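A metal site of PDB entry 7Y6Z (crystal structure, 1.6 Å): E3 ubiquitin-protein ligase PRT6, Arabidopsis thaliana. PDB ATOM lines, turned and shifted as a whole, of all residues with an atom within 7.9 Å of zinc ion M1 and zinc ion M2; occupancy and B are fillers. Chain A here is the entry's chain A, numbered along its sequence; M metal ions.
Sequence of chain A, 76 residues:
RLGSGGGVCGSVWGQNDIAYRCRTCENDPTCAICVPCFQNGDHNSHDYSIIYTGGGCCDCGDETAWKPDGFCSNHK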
ATOM      1  N   GLY A   7      18.747 -21.966   6.112  1.00  0.00           N
ATOM      2  CA  GLY A   7      19.635 -21.950   4.938  1.00  0.00           C
ATOM      3  C   GLY A   7      18.728 -21.755   3.715  1.00  0.00           C
ATOM      4  O   GLY A   7      17.531 -21.665   3.933  1.00  0.00           O
ATOM      5  N   VAL A   8      19.278 -21.687   2.487  1.00  0.00           N
ATOM      6  CA  VAL A   8      18.501 -21.651   1.239  1.00  0.00           C
ATOM      7  C   VAL A   8      18.902 -22.829   0.351  1.00  0.00           C
ATOM      8  O   VAL A   8      20.087 -22.968   0.003  1.00  0.00           O
ATOM      9  CB  VAL A   8      18.738 -20.348   0.479  1.00  0.00           C
ATOM     10  CG1 VAL A   8      20.277 -20.138   0.422  1.00  0.00           C
ATOM     11  CG2 VAL A   8      18.120 -20.477  -0.918  1.00  0.00           C
ATOM     12  N   CYS A   9      17.922 -23.625  -0.101  1.00  0.00           N
ATOM     13  CA  CYS A   9      18.271 -24.850  -0.806  1.00  0.00           C
ATOM     14  C   CYS A   9      18.928 -24.554  -2.145  1.00  0.00           C
ATOM     15  O   CYS A   9      18.420 -23.829  -2.984  1.00  0.00           O
ATOM     16  CB  CYS A   9      17.045 -25.759  -1.065  1.00  0.00           C
ATOM     17  SG  CYS A   9      17.552 -27.316  -1.948  1.00  0.00           S
ATOM     18  N   GLY A  10      20.050 -25.198  -2.388  1.00  0.00           N
ATOM     19  CA  GLY A  10      20.633 -24.987  -3.684  1.00  0.00           C
ATOM     20  C   GLY A  10      19.813 -25.550  -4.832  1.00  0.00           C
ATOM     21  O   GLY A  10      19.389 -24.830  -5.745  1.00  0.00           O
ATOM     22  N   SER A  11      19.634 -26.860  -4.760  1.00  0.00           N
ATOM     23  CA  SER A  11      19.255 -27.725  -5.854  1.00  0.00           C
ATOM     24  C   SER A  11      18.665 -27.177  -7.133  1.00  0.00           C
ATOM     25  O   SER A  11      17.597 -26.547  -7.178  1.00  0.00           O
ATOM     26  CB  SER A  11      18.319 -28.798  -5.307  1.00  0.00           C
ATOM     27  OG  SER A  11      18.842 -29.341  -4.118  1.00  0.00           O
ATOM     28  N   VAL A  12      19.374 -27.554  -8.195  1.00  0.00           N
ATOM     29  CA  VAL A  12      19.077 -27.221  -9.576  1.00  0.00           C
ATOM     30  C   VAL A  12      18.540 -28.441 -10.260  1.00  0.00           C
ATOM     31  O   VAL A  12      19.102 -29.542 -10.088  1.00  0.00           O
ATOM     32  CB  VAL A  12      20.357 -26.709 -10.265  1.00  0.00           C
ATOM     33  CG1 VAL A  12      20.138 -26.435 -11.740  1.00  0.00           C
ATOM     34  CG2 VAL A  12      20.805 -25.476  -9.543  1.00  0.00           C
ATOM     35  N   TRP A  13      17.470 -28.271 -11.056  1.00  0.00           N
ATOM     36  CA  TRP A  13      16.862 -29.313 -11.873  1.00  0.00           C
ATOM     37  C   TRP A  13      17.322 -29.149 -13.300  1.00  0.00           C
ATOM     38  O   TRP A  13      17.495 -28.045 -13.780  1.00  0.00           O
ATOM     39  CB  TRP A  13      15.319 -29.247 -11.853  1.00  0.00           C
ATOM     40  CG  TRP A  13      14.825 -29.251 -10.514  1.00  0.00           C
ATOM     41  CD1 TRP A  13      15.046 -30.200  -9.610  1.00  0.00           C
ATOM     42  CD2 TRP A  13      14.099 -28.216  -9.854  1.00  0.00           C
ATOM     43  NE1 TRP A  13      14.500 -29.861  -8.418  1.00  0.00           N
ATOM     44  CE2 TRP A  13      13.893 -28.660  -8.532  1.00  0.00           C
ATOM     45  CE3 TRP A  13      13.553 -26.994 -10.247  1.00  0.00           C
ATOM     46  CZ2 TRP A  13      13.175 -27.924  -7.599  1.00  0.00           C
ATOM     47  CZ3 TRP A  13      12.896 -26.242  -9.302  1.00  0.00           C
ATOM     48  CH2 TRP A  13      12.719 -26.713  -7.994  1.00  0.00           C
ATOM     49  N   ALA A  32       8.670 -23.746  -6.804  1.00  0.00           N
ATOM     50  CA  ALA A  32       8.707 -25.210  -6.703  1.00  0.00           C
ATOM     51  C   ALA A  32       9.761 -25.617  -5.685  1.00  0.00           C
ATOM     52  O   ALA A  32      10.678 -24.847  -5.411  1.00  0.00           O
ATOM     53  CB  ALA A  32       9.053 -25.912  -8.035  1.00  0.00           C
ATOM     54  N   ILE A  33       9.627 -26.827  -5.135  1.00  0.00           N
ATOM     55  CA  ILE A  33      10.698 -27.290  -4.250  1.00  0.00           C
ATOM     56  C   ILE A  33      11.129 -28.681  -4.651  1.00  0.00           C
ATOM     57  O   ILE A  33      10.311 -29.473  -5.148  1.00  0.00           O
ATOM     58  CB  ILE A  33      10.377 -27.250  -2.759  1.00  0.00           C
ATOM     59  CG1 ILE A  33       9.149 -28.072  -2.421  1.00  0.00           C
ATOM     60  CG2 ILE A  33      10.150 -25.746  -2.387  1.00  0.00           C
ATOM     61  CD1 ILE A  33       8.953 -28.170  -0.922  1.00  0.00           C
ATOM     62  N   CYS A  34      12.391 -28.970  -4.406  1.00  0.00           N
ATOM     63  CA  CYS A  34      12.908 -30.282  -4.772  1.00  0.00           C
ATOM     64  C   CYS A  34      12.254 -31.355  -3.935  1.00  0.00           C
ATOM     65  O   CYS A  34      11.759 -31.114  -2.833  1.00  0.00           O
ATOM     66  CB  CYS A  34      14.460 -30.303  -4.616  1.00  0.00           C
ATOM     67  SG  CYS A  34      15.147 -30.266  -2.991  1.00  0.00           S
ATOM     68  N   VAL A  35      12.351 -32.607  -4.403  1.00  0.00           N
ATOM     69  CA  VAL A  35      11.691 -33.707  -3.718  1.00  0.00           C
ATOM     70  C   VAL A  35      12.214 -33.853  -2.304  1.00  0.00           C
ATOM     71  O   VAL A  35      11.388 -34.065  -1.378  1.00  0.00           O
ATOM     72  CB  VAL A  35      11.854 -35.012  -4.515  1.00  0.00           C
ATOM     73  CG1 VAL A  35      11.303 -36.200  -3.704  1.00  0.00           C
ATOM     74  CG2 VAL A  35      11.169 -34.843  -5.820  1.00  0.00           C
ATOM     75  N   PRO A  36      13.531 -33.867  -2.032  1.00  0.00           N
ATOM     76  CA  PRO A  36      13.988 -34.014  -0.649  1.00  0.00           C
ATOM     77  C   PRO A  36      13.440 -32.923   0.283  1.00  0.00           C
ATOM     78  O   PRO A  36      13.054 -33.227   1.412  1.00  0.00           O
ATOM     79  CB  PRO A  36      15.513 -33.958  -0.759  1.00  0.00           C
ATOM     80  CG  PRO A  36      15.844 -34.032  -2.190  1.00  0.00           C
ATOM     81  CD  PRO A  36      14.651 -33.739  -2.990  1.00  0.00           C
ATOM     82  N   CYS A  37      13.419 -31.674  -0.159  1.00  0.00           N
ATOM     83  CA  CYS A  37      12.835 -30.639   0.703  1.00  0.00           C
ATOM     84  C   CYS A  37      11.332 -30.876   0.909  1.00  0.00           C
ATOM     85  O   CYS A  37      10.787 -30.623   2.006  1.00  0.00           O
ATOM     86  CB  CYS A  37      13.124 -29.241   0.141  1.00  0.00           C
ATOM     87  SG  CYS A  37      14.796 -28.671   0.081  1.00  0.00           S
ATOM     88  N   PHE A  38      10.611 -31.266  -0.137  1.00  0.00           N
ATOM     89  CA  PHE A  38       9.182 -31.603   0.062  1.00  0.00           C
ATOM     90  C   PHE A  38       9.017 -32.664   1.108  1.00  0.00           C
ATOM     91  O   PHE A  38       8.130 -32.618   1.960  1.00  0.00           O
ATOM     92  CB  PHE A  38       8.548 -32.106  -1.237  1.00  0.00           C
ATOM     93  CG  PHE A  38       7.078 -32.470  -1.096  1.00  0.00           C
ATOM     94  CD1 PHE A  38       6.096 -31.465  -1.158  1.00  0.00           C
ATOM     95  CD2 PHE A  38       6.681 -33.793  -0.886  1.00  0.00           C
ATOM     96  CE1 PHE A  38       4.753 -31.770  -1.073  1.00  0.00           C
ATOM     97  CE2 PHE A  38       5.318 -34.094  -0.772  1.00  0.00           C
ATOM     98  CZ  PHE A  38       4.372 -33.062  -0.864  1.00  0.00           C
ATOM     99  N   ASN A  40      11.010 -33.481   3.541  1.00  0.00           N
ATOM    100  CA  ASN A  40      11.422 -33.140   4.884  1.00  0.00           C
ATOM    101  C   ASN A  40      10.631 -31.948   5.452  1.00  0.00           C
ATOM    102  O   ASN A  40      11.041 -31.389   6.457  1.00  0.00           O
ATOM    103  CB  ASN A  40      12.923 -32.856   4.947  1.00  0.00           C
ATOM    104  CG  ASN A  40      13.747 -34.086   4.753  1.00  0.00           C
ATOM    105  OD1 ASN A  40      13.380 -35.162   5.158  1.00  0.00           O
ATOM    106  ND2 ASN A  40      14.899 -33.928   4.134  1.00  0.00           N
ATOM    107  N   GLY A  41       9.500 -31.609   4.840  1.00  0.00           N
ATOM    108  CA  GLY A  41       8.606 -30.619   5.362  1.00  0.00           C
ATOM    109  C   GLY A  41       7.240 -31.210   5.589  1.00  0.00           C
ATOM    110  O   GLY A  41       7.075 -32.422   5.512  1.00  0.00           O
ATOM    111  N   CYS A  57      15.333 -24.057  -9.991  1.00  0.00           N
ATOM    112  CA  CYS A  57      16.024 -24.262  -8.714  1.00  0.00           C
ATOM    113  C   CYS A  57      15.017 -24.272  -7.568  1.00  0.00           C
ATOM    114  O   CYS A  57      13.961 -23.655  -7.627  1.00  0.00           O
ATOM    115  CB  CYS A  57      17.128 -23.186  -8.483  1.00  0.00           C
ATOM    116  SG  CYS A  57      16.629 -21.491  -8.319  1.00  0.00           S
ATOM    117  N   CYS A  58      15.351 -25.022  -6.517  1.00  0.00           N
ATOM    118  CA  CYS A  58      14.435 -25.179  -5.383  1.00  0.00           C
ATOM    119  C   CYS A  58      14.321 -23.866  -4.608  1.00  0.00           C
ATOM    120  O   CYS A  58      15.331 -23.194  -4.355  1.00  0.00           O
ATOM    121  CB  CYS A  58      14.933 -26.307  -4.458  1.00  0.00           C
ATOM    122  SG  CYS A  58      13.976 -26.582  -2.965  1.00  0.00           S
ATOM    123  N   ASP A  59      13.097 -23.547  -4.194  1.00  0.00           N
ATOM    124  CA  ASP A  59      12.791 -22.291  -3.477  1.00  0.00           C
ATOM    125  C   ASP A  59      12.717 -22.479  -1.970  1.00  0.00           C
ATOM    126  O   ASP A  59      12.478 -21.530  -1.240  1.00  0.00           O
ATOM    127  CB  ASP A  59      11.473 -21.711  -3.973  1.00  0.00           C
ATOM    128  CG  ASP A  59      11.535 -21.284  -5.406  1.00  0.00           C
ATOM    129  OD1 ASP A  59      12.437 -20.497  -5.755  1.00  0.00           O
ATOM    130  OD2 ASP A  59      10.635 -21.678  -6.206  1.00  0.00           O
ATOM    131  N   CYS A  60      12.953 -23.671  -1.471  1.00  0.00           N
ATOM    132  CA  CYS A  60      12.906 -23.958  -0.053  1.00  0.00           C
ATOM    133  C   CYS A  60      13.984 -23.166   0.651  1.00  0.00           C
ATOM    134  O   CYS A  60      15.165 -23.214   0.265  1.00  0.00           O
ATOM    135  CB  CYS A  60      13.102 -25.437   0.249  1.00  0.00           C
ATOM    136  SG  CYS A  60      12.935 -25.911   1.890  1.00  0.00           S
ATOM    137  N   GLY A  61      13.553 -22.412   1.665  1.00  0.00           N
ATOM    138  CA  GLY A  61      14.425 -21.551   2.409  1.00  0.00           C
ATOM    139  C   GLY A  61      14.392 -20.122   1.972  1.00  0.00           C
ATOM    140  O   GLY A  61      14.909 -19.276   2.702  1.00  0.00           O
ATOM    141  N   ASP A  62      13.810 -19.833   0.791  1.00  0.00           N
ATOM    142  CA  ASP A  62      13.681 -18.475   0.271  1.00  0.00           C
ATOM    143  C   ASP A  62      12.284 -17.972   0.593  1.00  0.00           C
ATOM    144  O   ASP A  62      11.324 -18.340  -0.086  1.00  0.00           O
ATOM    145  CB  ASP A  62      13.968 -18.492  -1.235  1.00  0.00           C
ATOM    146  CG  ASP A  62      13.910 -17.128  -1.890  1.00  0.00           C
ATOM    147  OD1 ASP A  62      13.651 -16.106  -1.204  1.00  0.00           O
ATOM    148  OD2 ASP A  62      14.088 -17.059  -3.132  1.00  0.00           O
ATOM    149  N   TRP A  66       8.688 -18.783  -1.238  1.00  0.00           N
ATOM    150  CA  TRP A  66       8.004 -19.885  -0.590  1.00  0.00           C
ATOM    151  C   TRP A  66       7.641 -19.456   0.809  1.00  0.00           C
ATOM    152  O   TRP A  66       8.430 -18.807   1.499  1.00  0.00           O
ATOM    153  CB  TRP A  66       8.943 -21.090  -0.593  1.00  0.00           C
ATOM    154  CG  TRP A  66       8.335 -22.440  -0.423  1.00  0.00           C
ATOM    155  CD1 TRP A  66       8.293 -23.166   0.725  1.00  0.00           C
ATOM    156  CD2 TRP A  66       7.694 -23.259  -1.454  1.00  0.00           C
ATOM    157  NE1 TRP A  66       7.643 -24.359   0.494  1.00  0.00           N
ATOM    158  CE2 TRP A  66       7.291 -24.453  -0.835  1.00  0.00           C
ATOM    159  CE3 TRP A  66       7.486 -23.097  -2.812  1.00  0.00           C
ATOM    160  CZ2 TRP A  66       6.718 -25.509  -1.545  1.00  0.00           C
ATOM    161  CZ3 TRP A  66       6.856 -24.055  -3.520  1.00  0.00           C
ATOM    162  CH2 TRP A  66       6.458 -25.277  -2.877  1.00  0.00           C
ATOM    163  N   GLY A  70       6.189 -23.736   4.887  1.00  0.00           N
ATOM    164  CA  GLY A  70       6.516 -24.803   3.963  1.00  0.00           C
ATOM    165  C   GLY A  70       7.969 -25.137   3.794  1.00  0.00           C
ATOM    166  O   GLY A  70       8.284 -26.066   3.012  1.00  0.00           O
ATOM    167  N   PHE A  71       8.858 -24.502   4.547  1.00  0.00           N
ATOM    168  CA  PHE A  71      10.274 -24.852   4.561  1.00  0.00           C
ATOM    169  C   PHE A  71      10.472 -26.240   5.182  1.00  0.00           C
ATOM    170  O   PHE A  71       9.690 -26.688   6.039  1.00  0.00           O
ATOM    171  CB  PHE A  71      11.076 -23.853   5.384  1.00  0.00           C
ATOM    172  CG  PHE A  71      11.125 -22.461   4.818  1.00  0.00           C
ATOM    173  CD1 PHE A  71      11.671 -21.430   5.526  1.00  0.00           C
ATOM    174  CD2 PHE A  71      10.628 -22.202   3.537  1.00  0.00           C
ATOM    175  CE1 PHE A  71      11.691 -20.139   4.978  1.00  0.00           C
ATOM    176  CE2 PHE A  71      10.750 -21.012   2.958  1.00  0.00           C
ATOM    177  CZ  PHE A  71      11.278 -19.947   3.676  1.00  0.00           C
ATOM    178  N   CYS A  72      11.497 -26.928   4.687  1.00  0.00           N
ATOM    179  CA  CYS A  72      11.933 -28.189   5.254  1.00  0.00           C
ATOM    180  C   CYS A  72      12.767 -27.994   6.529  1.00  0.00           C
ATOM    181  O   CYS A  72      13.112 -26.881   6.931  1.00  0.00           O
ATOM    182  CB  CYS A  72      12.676 -29.068   4.219  1.00  0.00           C
ATOM    183  SG  CYS A  72      14.284 -28.756   3.905  1.00  0.00           S
ATOM    184  N   SER A  73      13.057 -29.144   7.174  1.00  0.00           N
ATOM    185  CA  SER A  73      13.899 -29.290   8.356  1.00  0.00           C
ATOM    186  C   SER A  73      15.255 -28.607   8.234  1.00  0.00           C
ATOM    187  O   SER A  73      15.763 -28.052   9.222  1.00  0.00           O
ATOM    188  CB  SER A  73      14.120 -30.794   8.631  1.00  0.00           C
ATOM    189  OG  SER A  73      15.372 -31.233   8.117  1.00  0.00           O
ATOM    190  N   ASN A  74      15.853 -28.619   7.047  1.00  0.00           N
ATOM    191  CA  ASN A  74      17.230 -28.166   6.873  1.00  0.00           C
ATOM    192  C   ASN A  74      17.352 -26.743   6.369  1.00  0.00           C
ATOM    193  O   ASN A  74      18.486 -26.236   6.260  1.00  0.00           O
ATOM    194  CB  ASN A  74      17.992 -29.091   5.908  1.00  0.00           C
ATOM    195  CG  ASN A  74      17.870 -30.568   6.284  1.00  0.00           C
ATOM    196  OD1 ASN A  74      18.170 -30.973   7.407  1.00  0.00           O
ATOM    197  ND2 ASN A  74      17.418 -31.381   5.319  1.00  0.00           N
ATOM    198  N   HIS A  75      16.228 -26.034   6.120  1.00  0.00           N
ATOM    199  CA  HIS A  75      16.332 -24.714   5.503  1.00  0.00           C
ATOM    200  C   HIS A  75      15.635 -23.652   6.315  1.00  0.00           C
ATOM    201  O   HIS A  75      15.134 -22.686   5.768  1.00  0.00           O
ATOM    202  CB  HIS A  75      15.856 -24.740   4.043  1.00  0.00           C
ATOM    203  CG  HIS A  75      16.732 -25.628   3.188  1.00  0.00           C
ATOM    204  ND1 HIS A  75      16.333 -26.858   2.698  1.00  0.00           N
ATOM    205  CD2 HIS A  75      18.042 -25.506   2.842  1.00  0.00           C
ATOM    206  CE1 HIS A  75      17.322 -27.410   2.038  1.00  0.00           C
ATOM    207  NE2 HIS A  75      18.391 -26.628   2.144  1.00  0.00           N
ATOM    208  N   LYS A  76      15.638 -23.805   7.644  1.00  0.00           N
ATOM    209  CA  LYS A  76      14.995 -22.825   8.510  1.00  0.00           C
ATOM    210  C   LYS A  76      16.006 -22.110   9.399  1.00  0.00           C
ATOM    211  O   LYS A  76      15.689 -21.019   9.948  1.00  0.00           O
ATOM    212  CB  LYS A  76      13.946 -23.502   9.365  1.00  0.00           C
ATOM    213  CG  LYS A  76      12.876 -24.113   8.614  1.00  0.00           C
ATOM    214  CD  LYS A  76      12.152 -25.055   9.551  1.00  0.00           C
ATOM    215  CE  LYS A  76      10.783 -25.445   9.063  1.00  0.00           C
ATOM    216  NZ  LYS A  76       9.976 -26.176  10.124  1.00  0.00           N
HETATM  217 ZN    ZN M   1      15.342 -28.161  -2.003  1.00  0.00          ZN
HETATM  218 ZN    ZN M   2      14.544 -27.387   2.149  1.00  0.00          ZN
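The backbone NH (N) of Cys 58 sits at hydrogen-bond distance from the backbone carbonyl oxygen (O) of Ser 11 (2.8 Å). The side-chain sulfur of Cys 58 lies close to the backbone NH of Cys 60 (3.4 Å). SG of Cys 72 sits close to N of Asn 74 (3.5 Å). The side-chain sulfur (SG) of Cys 9 lies close to the side-chain hydroxyl (OG) of Ser 11, 3.2 Å away. The backbone carbonyl oxygen (O) of Cys 60 lies within hydrogen-bond range of the backbone NH (N) of Cys 9 (2.8 Å).
Zinc ion M1 is bound by the side-chain sulfur (SG) of Cys 37, the side-chain sulfur (SG) of Cys 58, the side-chain sulfur (SG) of Cys 34 and the side-chain sulfur (SG) of Cys 9. Zinc ion M1 has four donor atoms within binding distance.
A ring nitrogen (ND1) of His 75 is bound to zinc ion M2. Zinc ion M2 is bound by SG of Cys 60, 2.2 Å away. SG of Cys 72 binds zinc ion M2 (2.2 Å). Zinc ion M2 is bound by SG of Cys 37.
Of the 30 residues printed, 4 come within 4 Å of zinc ion M1. The nearest printed residue that does not touch zinc ion M1 is Cys 60 (4.2 Å).
The nearest printed residue that does not touch zinc ion M2 is Cys 9 (4.4 Å).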
